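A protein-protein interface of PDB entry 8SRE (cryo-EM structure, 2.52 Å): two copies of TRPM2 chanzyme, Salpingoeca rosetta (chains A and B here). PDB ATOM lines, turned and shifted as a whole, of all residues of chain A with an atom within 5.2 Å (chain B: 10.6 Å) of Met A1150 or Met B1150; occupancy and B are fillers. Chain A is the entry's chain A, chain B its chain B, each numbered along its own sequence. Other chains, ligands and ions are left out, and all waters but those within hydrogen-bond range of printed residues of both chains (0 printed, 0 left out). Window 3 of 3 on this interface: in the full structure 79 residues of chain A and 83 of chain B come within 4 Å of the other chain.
Of the printed residues of chain B, Met A1150 touches Ala B1146 (3.6 Å), Met B1149 (3.5 Å) and Met B1150 (3.4 Å).
Met B1150 touches just one residue of chain A: Met A1150 (3.4 Å).
No residue of chain B comes within 4 Å of Gly A1148.
No residue of chain B comes within 4 Å of Asp A1151.
No residue of chain B comes within 4 Å of Gln A1152.
Leu A1154 touches just these residues of chain B: Gln B1152 and Leu B1153.
Of the printed residues of chain A, Leu B1153 touches Leu A1153 and Leu A1154.
Printed residues of chain A within 4 Å of Asn B1142: Met A1147 (3.4 Å).
Of the printed residues of chain A, Met B1149 touches Met A1150.
Asp B1151 touches none of the printed residues of chain A.
Met A1149 touches none of the printed residues of chain B.
The nearest printed residue of chain A that does not touch Met B1150 is Leu A1154 (7.1 Å).
Of the 10 printed residues of chain A, 4 touch a printed residue of chain B.
Hydrophobic or aromatic side chains of chain A within 4 Å of the printed part of chain B: Met A1147, Met A1150, Leu A1153 and Leu A1154.
Of the 18 printed residues of chain B, 7 touch a printed residue of chain A.
Among the printed residues, no Asp or Glu carboxylate lies within 4 Å of a Lys or Arg side-chain nitrogen of the other chain.
The backbone carbonyl oxygen of Gln B1152 is in hydrogen-bond range of a ring nitrogen (ND1) of His B1156 (3.0 Å).
The backbone carbonyl oxygen of Gly B1148 lies within hydrogen-bond range of the side-chain amide nitrogen of Gln B1152 (2.9 Å).
O of Ala B1146 lies close to SD of Met A1150.
The backbone carbonyl oxygen (O) of Asn B1142 sits close to the side-chain sulfur (SD) of Met A1147 (3.7 Å).
Met A1150 touches Met B1149, but with the chains exchanged Met A1149 does not touch Met B1150 (9.3 Å).
Met A1150 touches its own counterpart, Met B1150.
Leu B1153 touches its own counterpart, Leu A1153.
Leu A1154 touches Gln B1152, but with the chains exchanged Gln A1152 does not touch Leu B1154 (12.2 Å).
10 positions are printed for both chains.
Among the printed residues, merely in contact across the chains: Met A1147 with Gln B1145 (3.6 Å), Met A1150 with Met B1149 (3.5 Å), Met A1150 with Met B1150 (3.4 Å), Leu A1153 with Leu B1153 (3.8 Å), Leu A1154 with Gln B1152 (3.8 Å) and Leu A1154 with Leu B1153 (3.9 Å).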
ATOM      1  N   ALA A1146     -19.025 -33.910   2.076  1.00  0.00           N
ATOM      2  CA  ALA A1146     -19.838 -33.882   3.297  1.00  0.00           C
ATOM      3  C   ALA A1146     -20.479 -32.509   3.516  1.00  0.00           C
ATOM      4  O   ALA A1146     -21.619 -32.443   3.996  1.00  0.00           O
ATOM      5  CB  ALA A1146     -19.027 -34.324   4.513  1.00  0.00           C
ATOM      6  N   MET A1147     -19.760 -31.425   3.274  1.00  0.00           N
ATOM      7  CA  MET A1147     -20.442 -30.120   3.406  1.00  0.00           C
ATOM      8  C   MET A1147     -21.484 -29.995   2.292  1.00  0.00           C
ATOM      9  O   MET A1147     -22.563 -29.479   2.576  1.00  0.00           O
ATOM     10  CB  MET A1147     -19.463 -28.954   3.328  1.00  0.00           C
ATOM     11  CG  MET A1147     -18.086 -29.277   3.819  1.00  0.00           C
ATOM     12  SD  MET A1147     -18.024 -29.251   5.611  1.00  0.00           S
ATOM     13  CE  MET A1147     -17.576 -27.537   5.873  1.00  0.00           C
ATOM     14  N   GLY A1148     -21.172 -30.415   1.065  1.00  0.00           N
ATOM     15  CA  GLY A1148     -22.205 -30.391   0.017  1.00  0.00           C
ATOM     16  C   GLY A1148     -23.505 -31.041   0.473  1.00  0.00           C
ATOM     17  O   GLY A1148     -24.607 -30.516   0.227  1.00  0.00           O
ATOM     18  N   MET A1149     -23.373 -32.203   1.141  1.00  0.00           N
ATOM     19  CA  MET A1149     -24.521 -32.916   1.707  1.00  0.00           C
ATOM     20  C   MET A1149     -25.173 -32.149   2.865  1.00  0.00           C
ATOM     21  O   MET A1149     -26.402 -32.225   2.999  1.00  0.00           O
ATOM     22  CB  MET A1149     -24.166 -34.350   2.088  1.00  0.00           C
ATOM     23  CG  MET A1149     -23.879 -35.191   0.858  1.00  0.00           C
ATOM     24  SD  MET A1149     -23.377 -36.890   1.150  1.00  0.00           S
ATOM     25  CE  MET A1149     -22.373 -37.183  -0.290  1.00  0.00           C
ATOM     26  N   MET A1150     -24.417 -31.445   3.694  1.00  0.00           N
ATOM     27  CA  MET A1150     -25.115 -30.656   4.735  1.00  0.00           C
ATOM     28  C   MET A1150     -25.838 -29.472   4.080  1.00  0.00           C
ATOM     29  O   MET A1150     -26.938 -29.169   4.532  1.00  0.00           O
ATOM     30  CB  MET A1150     -24.164 -30.177   5.825  1.00  0.00           C
ATOM     31  CG  MET A1150     -23.601 -31.287   6.657  1.00  0.00           C
ATOM     32  SD  MET A1150     -22.422 -30.698   7.872  1.00  0.00           S
ATOM     33  CE  MET A1150     -21.932 -32.254   8.609  1.00  0.00           C
ATOM     34  N   ASP A1151     -25.257 -28.826   3.065  1.00  0.00           N
ATOM     35  CA  ASP A1151     -25.980 -27.769   2.351  1.00  0.00           C
ATOM     36  C   ASP A1151     -27.333 -28.244   1.828  1.00  0.00           C
ATOM     37  O   ASP A1151     -28.329 -27.508   1.942  1.00  0.00           O
ATOM     38  CB  ASP A1151     -25.127 -27.220   1.209  1.00  0.00           C
ATOM     39  CG  ASP A1151     -23.938 -26.425   1.706  1.00  0.00           C
ATOM     40  OD1 ASP A1151     -23.979 -25.958   2.863  1.00  0.00           O
ATOM     41  OD2 ASP A1151     -22.964 -26.262   0.940  1.00  0.00           O
ATOM     42  N   GLN A1152     -27.361 -29.462   1.232  1.00  0.00           N
ATOM     43  CA  GLN A1152     -28.611 -30.092   0.772  1.00  0.00           C
ATOM     44  C   GLN A1152     -29.599 -30.378   1.911  1.00  0.00           C
ATOM     45  O   GLN A1152     -30.811 -30.133   1.746  1.00  0.00           O
ATOM     46  CB  GLN A1152     -28.300 -31.377   0.007  1.00  0.00           C
ATOM     47  CG  GLN A1152     -27.567 -31.153  -1.302  1.00  0.00           C
ATOM     48  CD  GLN A1152     -26.689 -32.323  -1.686  1.00  0.00           C
ATOM     49  OE1 GLN A1152     -27.126 -33.474  -1.668  1.00  0.00           O
ATOM     50  NE2 GLN A1152     -25.443 -32.038  -2.041  1.00  0.00           N
ATOM     51  N   LEU A1153     -29.091 -30.921   3.046  1.00  0.00           N
ATOM     52  CA  LEU A1153     -29.905 -31.200   4.243  1.00  0.00           C
ATOM     53  C   LEU A1153     -30.500 -29.937   4.859  1.00  0.00           C
ATOM     54  O   LEU A1153     -31.692 -29.917   5.185  1.00  0.00           O
ATOM     55  CB  LEU A1153     -29.114 -31.955   5.313  1.00  0.00           C
ATOM     56  CG  LEU A1153     -28.675 -33.412   5.193  1.00  0.00           C
ATOM     57  CD1 LEU A1153     -27.655 -33.728   6.263  1.00  0.00           C
ATOM     58  CD2 LEU A1153     -29.850 -34.327   5.317  1.00  0.00           C
ATOM     59  N   LEU A1154     -29.681 -28.868   4.974  1.00  0.00           N
ATOM     60  CA  LEU A1154     -30.098 -27.589   5.559  1.00  0.00           C
ATOM     61  C   LEU A1154     -31.122 -26.860   4.693  1.00  0.00           C
ATOM     62  O   LEU A1154     -32.053 -26.237   5.233  1.00  0.00           O
ATOM     63  CB  LEU A1154     -28.870 -26.718   5.796  1.00  0.00           C
ATOM     64  CG  LEU A1154     -29.047 -25.521   6.722  1.00  0.00           C
ATOM     65  CD1 LEU A1154     -29.130 -25.996   8.158  1.00  0.00           C
ATOM     66  CD2 LEU A1154     -27.894 -24.551   6.543  1.00  0.00           C
ATOM     67  N   GLU A1155     -30.951 -26.951   3.356  1.00  0.00           N
ATOM     68  CA  GLU A1155     -31.901 -26.426   2.368  1.00  0.00           C
ATOM     69  C   GLU A1155     -33.269 -27.099   2.472  1.00  0.00           C
ATOM     70  O   GLU A1155     -34.314 -26.418   2.438  1.00  0.00           O
ATOM     71  CB  GLU A1155     -31.288 -26.601   0.975  1.00  0.00           C
ATOM     72  CG  GLU A1155     -32.230 -26.725  -0.215  1.00  0.00           C
ATOM     73  CD  GLU A1155     -33.000 -25.478  -0.542  1.00  0.00           C
ATOM     74  OE1 GLU A1155     -32.497 -24.362  -0.295  1.00  0.00           O
ATOM     75  OE2 GLU A1155     -34.090 -25.632  -1.130  1.00  0.00           O
ATOM     76  N   ASP B1141     -10.373 -27.388  10.095  1.00  0.00           N
ATOM     77  CA  ASP B1141     -11.275 -26.221  10.062  1.00  0.00           C
ATOM     78  C   ASP B1141     -12.625 -26.561   9.429  1.00  0.00           C
ATOM     79  O   ASP B1141     -13.663 -26.017   9.841  1.00  0.00           O
ATOM     80  CB  ASP B1141     -10.634 -25.034   9.342  1.00  0.00           C
ATOM     81  CG  ASP B1141      -9.335 -24.592   9.974  1.00  0.00           C
ATOM     82  OD1 ASP B1141      -9.023 -25.055  11.091  1.00  0.00           O
ATOM     83  OD2 ASP B1141      -8.616 -23.784   9.349  1.00  0.00           O
ATOM     84  N   ASN B1142     -12.597 -27.396   8.374  1.00  0.00           N
ATOM     85  CA  ASN B1142     -13.806 -27.872   7.697  1.00  0.00           C
ATOM     86  C   ASN B1142     -14.669 -28.741   8.619  1.00  0.00           C
ATOM     87  O   ASN B1142     -15.900 -28.683   8.550  1.00  0.00           O
ATOM     88  CB  ASN B1142     -13.450 -28.590   6.406  1.00  0.00           C
ATOM     89  CG  ASN B1142     -13.095 -27.643   5.289  1.00  0.00           C
ATOM     90  OD1 ASN B1142     -13.451 -26.467   5.318  1.00  0.00           O
ATOM     91  ND2 ASN B1142     -12.395 -28.154   4.285  1.00  0.00           N
ATOM     92  N   VAL B1143     -14.036 -29.603   9.430  1.00  0.00           N
ATOM     93  CA  VAL B1143     -14.742 -30.459  10.397  1.00  0.00           C
ATOM     94  C   VAL B1143     -15.374 -29.585  11.519  1.00  0.00           C
ATOM     95  O   VAL B1143     -16.468 -29.904  12.031  1.00  0.00           O
ATOM     96  CB  VAL B1143     -13.767 -31.588  10.821  1.00  0.00           C
ATOM     97  CG1 VAL B1143     -14.136 -32.297  12.059  1.00  0.00           C
ATOM     98  CG2 VAL B1143     -13.764 -32.653   9.743  1.00  0.00           C
ATOM     99  N   VAL B1144     -14.693 -28.479  11.897  1.00  0.00           N
ATOM    100  CA  VAL B1144     -15.229 -27.467  12.833  1.00  0.00           C
ATOM    101  C   VAL B1144     -16.483 -26.774  12.234  1.00  0.00           C
ATOM    102  O   VAL B1144     -17.501 -26.558  12.928  1.00  0.00           O
ATOM    103  CB  VAL B1144     -14.096 -26.486  13.218  1.00  0.00           C
ATOM    104  CG1 VAL B1144     -14.581 -25.182  13.847  1.00  0.00           C
ATOM    105  CG2 VAL B1144     -13.165 -27.160  14.204  1.00  0.00           C
ATOM    106  N   GLN B1145     -16.406 -26.388  10.944  1.00  0.00           N
ATOM    107  CA  GLN B1145     -17.550 -25.830  10.201  1.00  0.00           C
ATOM    108  C   GLN B1145     -18.708 -26.844  10.044  1.00  0.00           C
ATOM    109  O   GLN B1145     -19.892 -26.455  10.055  1.00  0.00           O
ATOM    110  CB  GLN B1145     -17.056 -25.328   8.845  1.00  0.00           C
ATOM    111  CG  GLN B1145     -17.983 -24.371   8.145  1.00  0.00           C
ATOM    112  CD  GLN B1145     -17.421 -23.887   6.824  1.00  0.00           C
ATOM    113  OE1 GLN B1145     -16.283 -24.193   6.473  1.00  0.00           O
ATOM    114  NE2 GLN B1145     -18.221 -23.132   6.081  1.00  0.00           N
ATOM    115  N   ALA B1146     -18.355 -28.139   9.912  1.00  0.00           N
ATOM    116  CA  ALA B1146     -19.297 -29.263   9.878  1.00  0.00           C
ATOM    117  C   ALA B1146     -20.062 -29.399  11.197  1.00  0.00           C
ATOM    118  O   ALA B1146     -21.249 -29.750  11.175  1.00  0.00           O
ATOM    119  CB  ALA B1146     -18.593 -30.565   9.499  1.00  0.00           C
ATOM    120  N   MET B1147     -19.406 -29.228  12.333  1.00  0.00           N
ATOM    121  CA  MET B1147     -20.197 -29.274  13.581  1.00  0.00           C
ATOM    122  C   MET B1147     -21.117 -28.051  13.625  1.00  0.00           C
ATOM    123  O   MET B1147     -22.257 -28.211  14.058  1.00  0.00           O
ATOM    124  CB  MET B1147     -19.307 -29.293  14.819  1.00  0.00           C
ATOM    125  CG  MET B1147     -17.972 -29.935  14.604  1.00  0.00           C
ATOM    126  SD  MET B1147     -18.109 -31.723  14.635  1.00  0.00           S
ATOM    127  CE  MET B1147     -17.825 -32.017  16.378  1.00  0.00           C
ATOM    128  N   GLY B1148     -20.640 -26.870  13.231  1.00  0.00           N
ATOM    129  CA  GLY B1148     -21.550 -25.714  13.176  1.00  0.00           C
ATOM    130  C   GLY B1148     -22.839 -26.030  12.427  1.00  0.00           C
ATOM    131  O   GLY B1148     -23.944 -25.661  12.865  1.00  0.00           O
ATOM    132  N   MET B1149     -22.693 -26.719  11.279  1.00  0.00           N
ATOM    133  CA  MET B1149     -23.837 -27.163  10.480  1.00  0.00           C
ATOM    134  C   MET B1149     -24.670 -28.235  11.194  1.00  0.00           C
ATOM    135  O   MET B1149     -25.896 -28.234  11.024  1.00  0.00           O
ATOM    136  CB  MET B1149     -23.419 -27.592   9.077  1.00  0.00           C
ATOM    137  CG  MET B1149     -22.934 -26.408   8.260  1.00  0.00           C
ATOM    138  SD  MET B1149     -22.338 -26.768   6.605  1.00  0.00           S
ATOM    139  CE  MET B1149     -21.163 -25.450   6.390  1.00  0.00           C
ATOM    140  N   MET B1150     -24.066 -29.135  11.954  1.00  0.00           N
ATOM    141  CA  MET B1150     -24.933 -30.087  12.687  1.00  0.00           C
ATOM    142  C   MET B1150     -25.667 -29.346  13.812  1.00  0.00           C
ATOM    143  O   MET B1150     -26.830 -29.673  14.030  1.00  0.00           O
ATOM    144  CB  MET B1150     -24.147 -31.270  13.238  1.00  0.00           C
ATOM    145  CG  MET B1150     -23.595 -32.169  12.175  1.00  0.00           C
ATOM    146  SD  MET B1150     -22.605 -33.501  12.854  1.00  0.00           S
ATOM    147  CE  MET B1150     -22.081 -34.300  11.340  1.00  0.00           C
ATOM    148  N   ASP B1151     -25.030 -28.396  14.501  1.00  0.00           N
ATOM    149  CA  ASP B1151     -25.748 -27.599  15.498  1.00  0.00           C
ATOM    150  C   ASP B1151     -26.995 -26.933  14.921  1.00  0.00           C
ATOM    151  O   ASP B1151     -28.052 -26.931  15.578  1.00  0.00           O
ATOM    152  CB  ASP B1151     -24.820 -26.552  16.112  1.00  0.00           C
ATOM    153  CG  ASP B1151     -23.758 -27.169  16.996  1.00  0.00           C
ATOM    154  OD1 ASP B1151     -23.961 -28.310  17.459  1.00  0.00           O
ATOM    155  OD2 ASP B1151     -22.721 -26.513  17.233  1.00  0.00           O
ATOM    156  N   GLN B1152     -26.864 -26.348  13.704  1.00  0.00           N
ATOM    157  CA  GLN B1152     -28.004 -25.760  12.980  1.00  0.00           C
ATOM    158  C   GLN B1152     -29.087 -26.786  12.618  1.00  0.00           C
ATOM    159  O   GLN B1152     -30.289 -26.488  12.769  1.00  0.00           O
ATOM    160  CB  GLN B1152     -27.514 -25.045  11.722  1.00  0.00           C
ATOM    161  CG  GLN B1152     -26.661 -23.822  12.001  1.00  0.00           C
ATOM    162  CD  GLN B1152     -25.659 -23.547  10.902  1.00  0.00           C
ATOM    163  OE1 GLN B1152     -26.006 -23.527   9.722  1.00  0.00           O
ATOM    164  NE2 GLN B1152     -24.406 -23.328  11.283  1.00  0.00           N
ATOM    165  N   LEU B1153     -28.666 -27.975  12.116  1.00  0.00           N
ATOM    166  CA  LEU B1153     -29.583 -29.078  11.776  1.00  0.00           C
ATOM    167  C   LEU B1153     -30.337 -29.614  12.989  1.00  0.00           C
ATOM    168  O   LEU B1153     -31.556 -29.807  12.917  1.00  0.00           O
ATOM    169  CB  LEU B1153     -28.859 -30.235  11.085  1.00  0.00           C
ATOM    170  CG  LEU B1153     -28.299 -30.175   9.664  1.00  0.00           C
ATOM    171  CD1 LEU B1153     -27.383 -31.354   9.428  1.00  0.00           C
ATOM    172  CD2 LEU B1153     -29.408 -30.178   8.661  1.00  0.00           C
ATOM    173  N   LEU B1154     -29.620 -29.808  14.118  1.00  0.00           N
ATOM    174  CA  LEU B1154     -30.196 -30.334  15.361  1.00  0.00           C
ATOM    175  C   LEU B1154     -31.172 -29.354  16.009  1.00  0.00           C
ATOM    176  O   LEU B1154     -32.202 -29.784  16.558  1.00  0.00           O
ATOM    177  CB  LEU B1154     -29.072 -30.697  16.325  1.00  0.00           C
ATOM    178  CG  LEU B1154     -29.441 -31.587  17.505  1.00  0.00           C
ATOM    179  CD1 LEU B1154     -29.645 -33.010  17.024  1.00  0.00           C
ATOM    180  CD2 LEU B1154     -28.353 -31.527  18.561  1.00  0.00           C
ATOM    181  N   GLU B1155     -30.848 -28.044  15.931  1.00  0.00           N
ATOM    182  CA  GLU B1155     -31.722 -26.954  16.381  1.00  0.00           C
ATOM    183  C   GLU B1155     -33.036 -26.913  15.605  1.00  0.00           C
ATOM    184  O   GLU B1155     -34.121 -26.759  16.204  1.00  0.00           O
ATOM    185  CB  GLU B1155     -30.947 -25.638  16.253  1.00  0.00           C
ATOM    186  CG  GLU B1155     -31.741 -24.353  16.058  1.00  0.00           C
ATOM    187  CD  GLU B1155     -32.563 -23.933  17.241  1.00  0.00           C
ATOM    188  OE1 GLU B1155     -32.177 -24.224  18.393  1.00  0.00           O
ATOM    189  OE2 GLU B1155     -33.566 -23.231  17.003  1.00  0.00           O
ATOM    190  N   HIS B1156     -32.940 -27.051  14.269  1.00  0.00           N
ATOM    191  CA  HIS B1156     -34.110 -27.096  13.395  1.00  0.00           C
ATOM    192  C   HIS B1156     -34.987 -28.351  13.635  1.00  0.00           C
ATOM    193  O   HIS B1156     -36.228 -28.247  13.543  1.00  0.00           O
ATOM    194  CB  HIS B1156     -33.630 -26.923  11.962  1.00  0.00           C
ATOM    195  CG  HIS B1156     -33.406 -25.502  11.554  1.00  0.00           C
ATOM    196  ND1 HIS B1156     -32.591 -24.642  12.259  1.00  0.00           N
ATOM    197  CD2 HIS B1156     -33.868 -24.796  10.495  1.00  0.00           C
ATOM    198  CE1 HIS B1156     -32.575 -23.465  11.662  1.00  0.00           C
ATOM    199  NE2 HIS B1156     -33.341 -23.532  10.588  1.00  0.00           N
ATOM    200  N   MET B1157     -34.356 -29.525  13.913  1.00  0.00           N
ATOM    201  CA  MET B1157     -35.069 -30.766  14.296  1.00  0.00           C
ATOM    202  C   MET B1157     -35.882 -30.612  15.583  1.00  0.00           C
ATOM    203  O   MET B1157     -37.016 -31.115  15.661  1.00  0.00           O
ATOM    204  CB  MET B1157     -34.142 -31.975  14.467  1.00  0.00           C
ATOM    205  CG  MET B1157     -33.432 -32.544  13.267  1.00  0.00           C
ATOM    206  SD  MET B1157     -34.552 -33.140  12.013  1.00  0.00           S
ATOM    207  CE  MET B1157     -35.229 -34.512  12.816  1.00  0.00           C
ATOM    208  N   ILE B1158     -35.265 -30.014  16.626  1.00  0.00           N
ATOM    209  CA  ILE B1158     -35.910 -29.782  17.930  1.00  0.00           C
ATOM    210  C   ILE B1158     -37.098 -28.809  17.797  1.00  0.00           C
ATOM    211  O   ILE B1158     -38.146 -29.015  18.451  1.00  0.00           O
ATOM    212  CB  ILE B1158     -34.817 -29.350  18.947  1.00  0.00           C
ATOM    213  CG1 ILE B1158     -33.958 -30.567  19.308  1.00  0.00           C
ATOM    214  CG2 ILE B1158     -35.348 -28.780  20.272  1.00  0.00           C
ATOM    215  CD1 ILE B1158     -32.706 -30.260  20.130  1.00  0.00           C
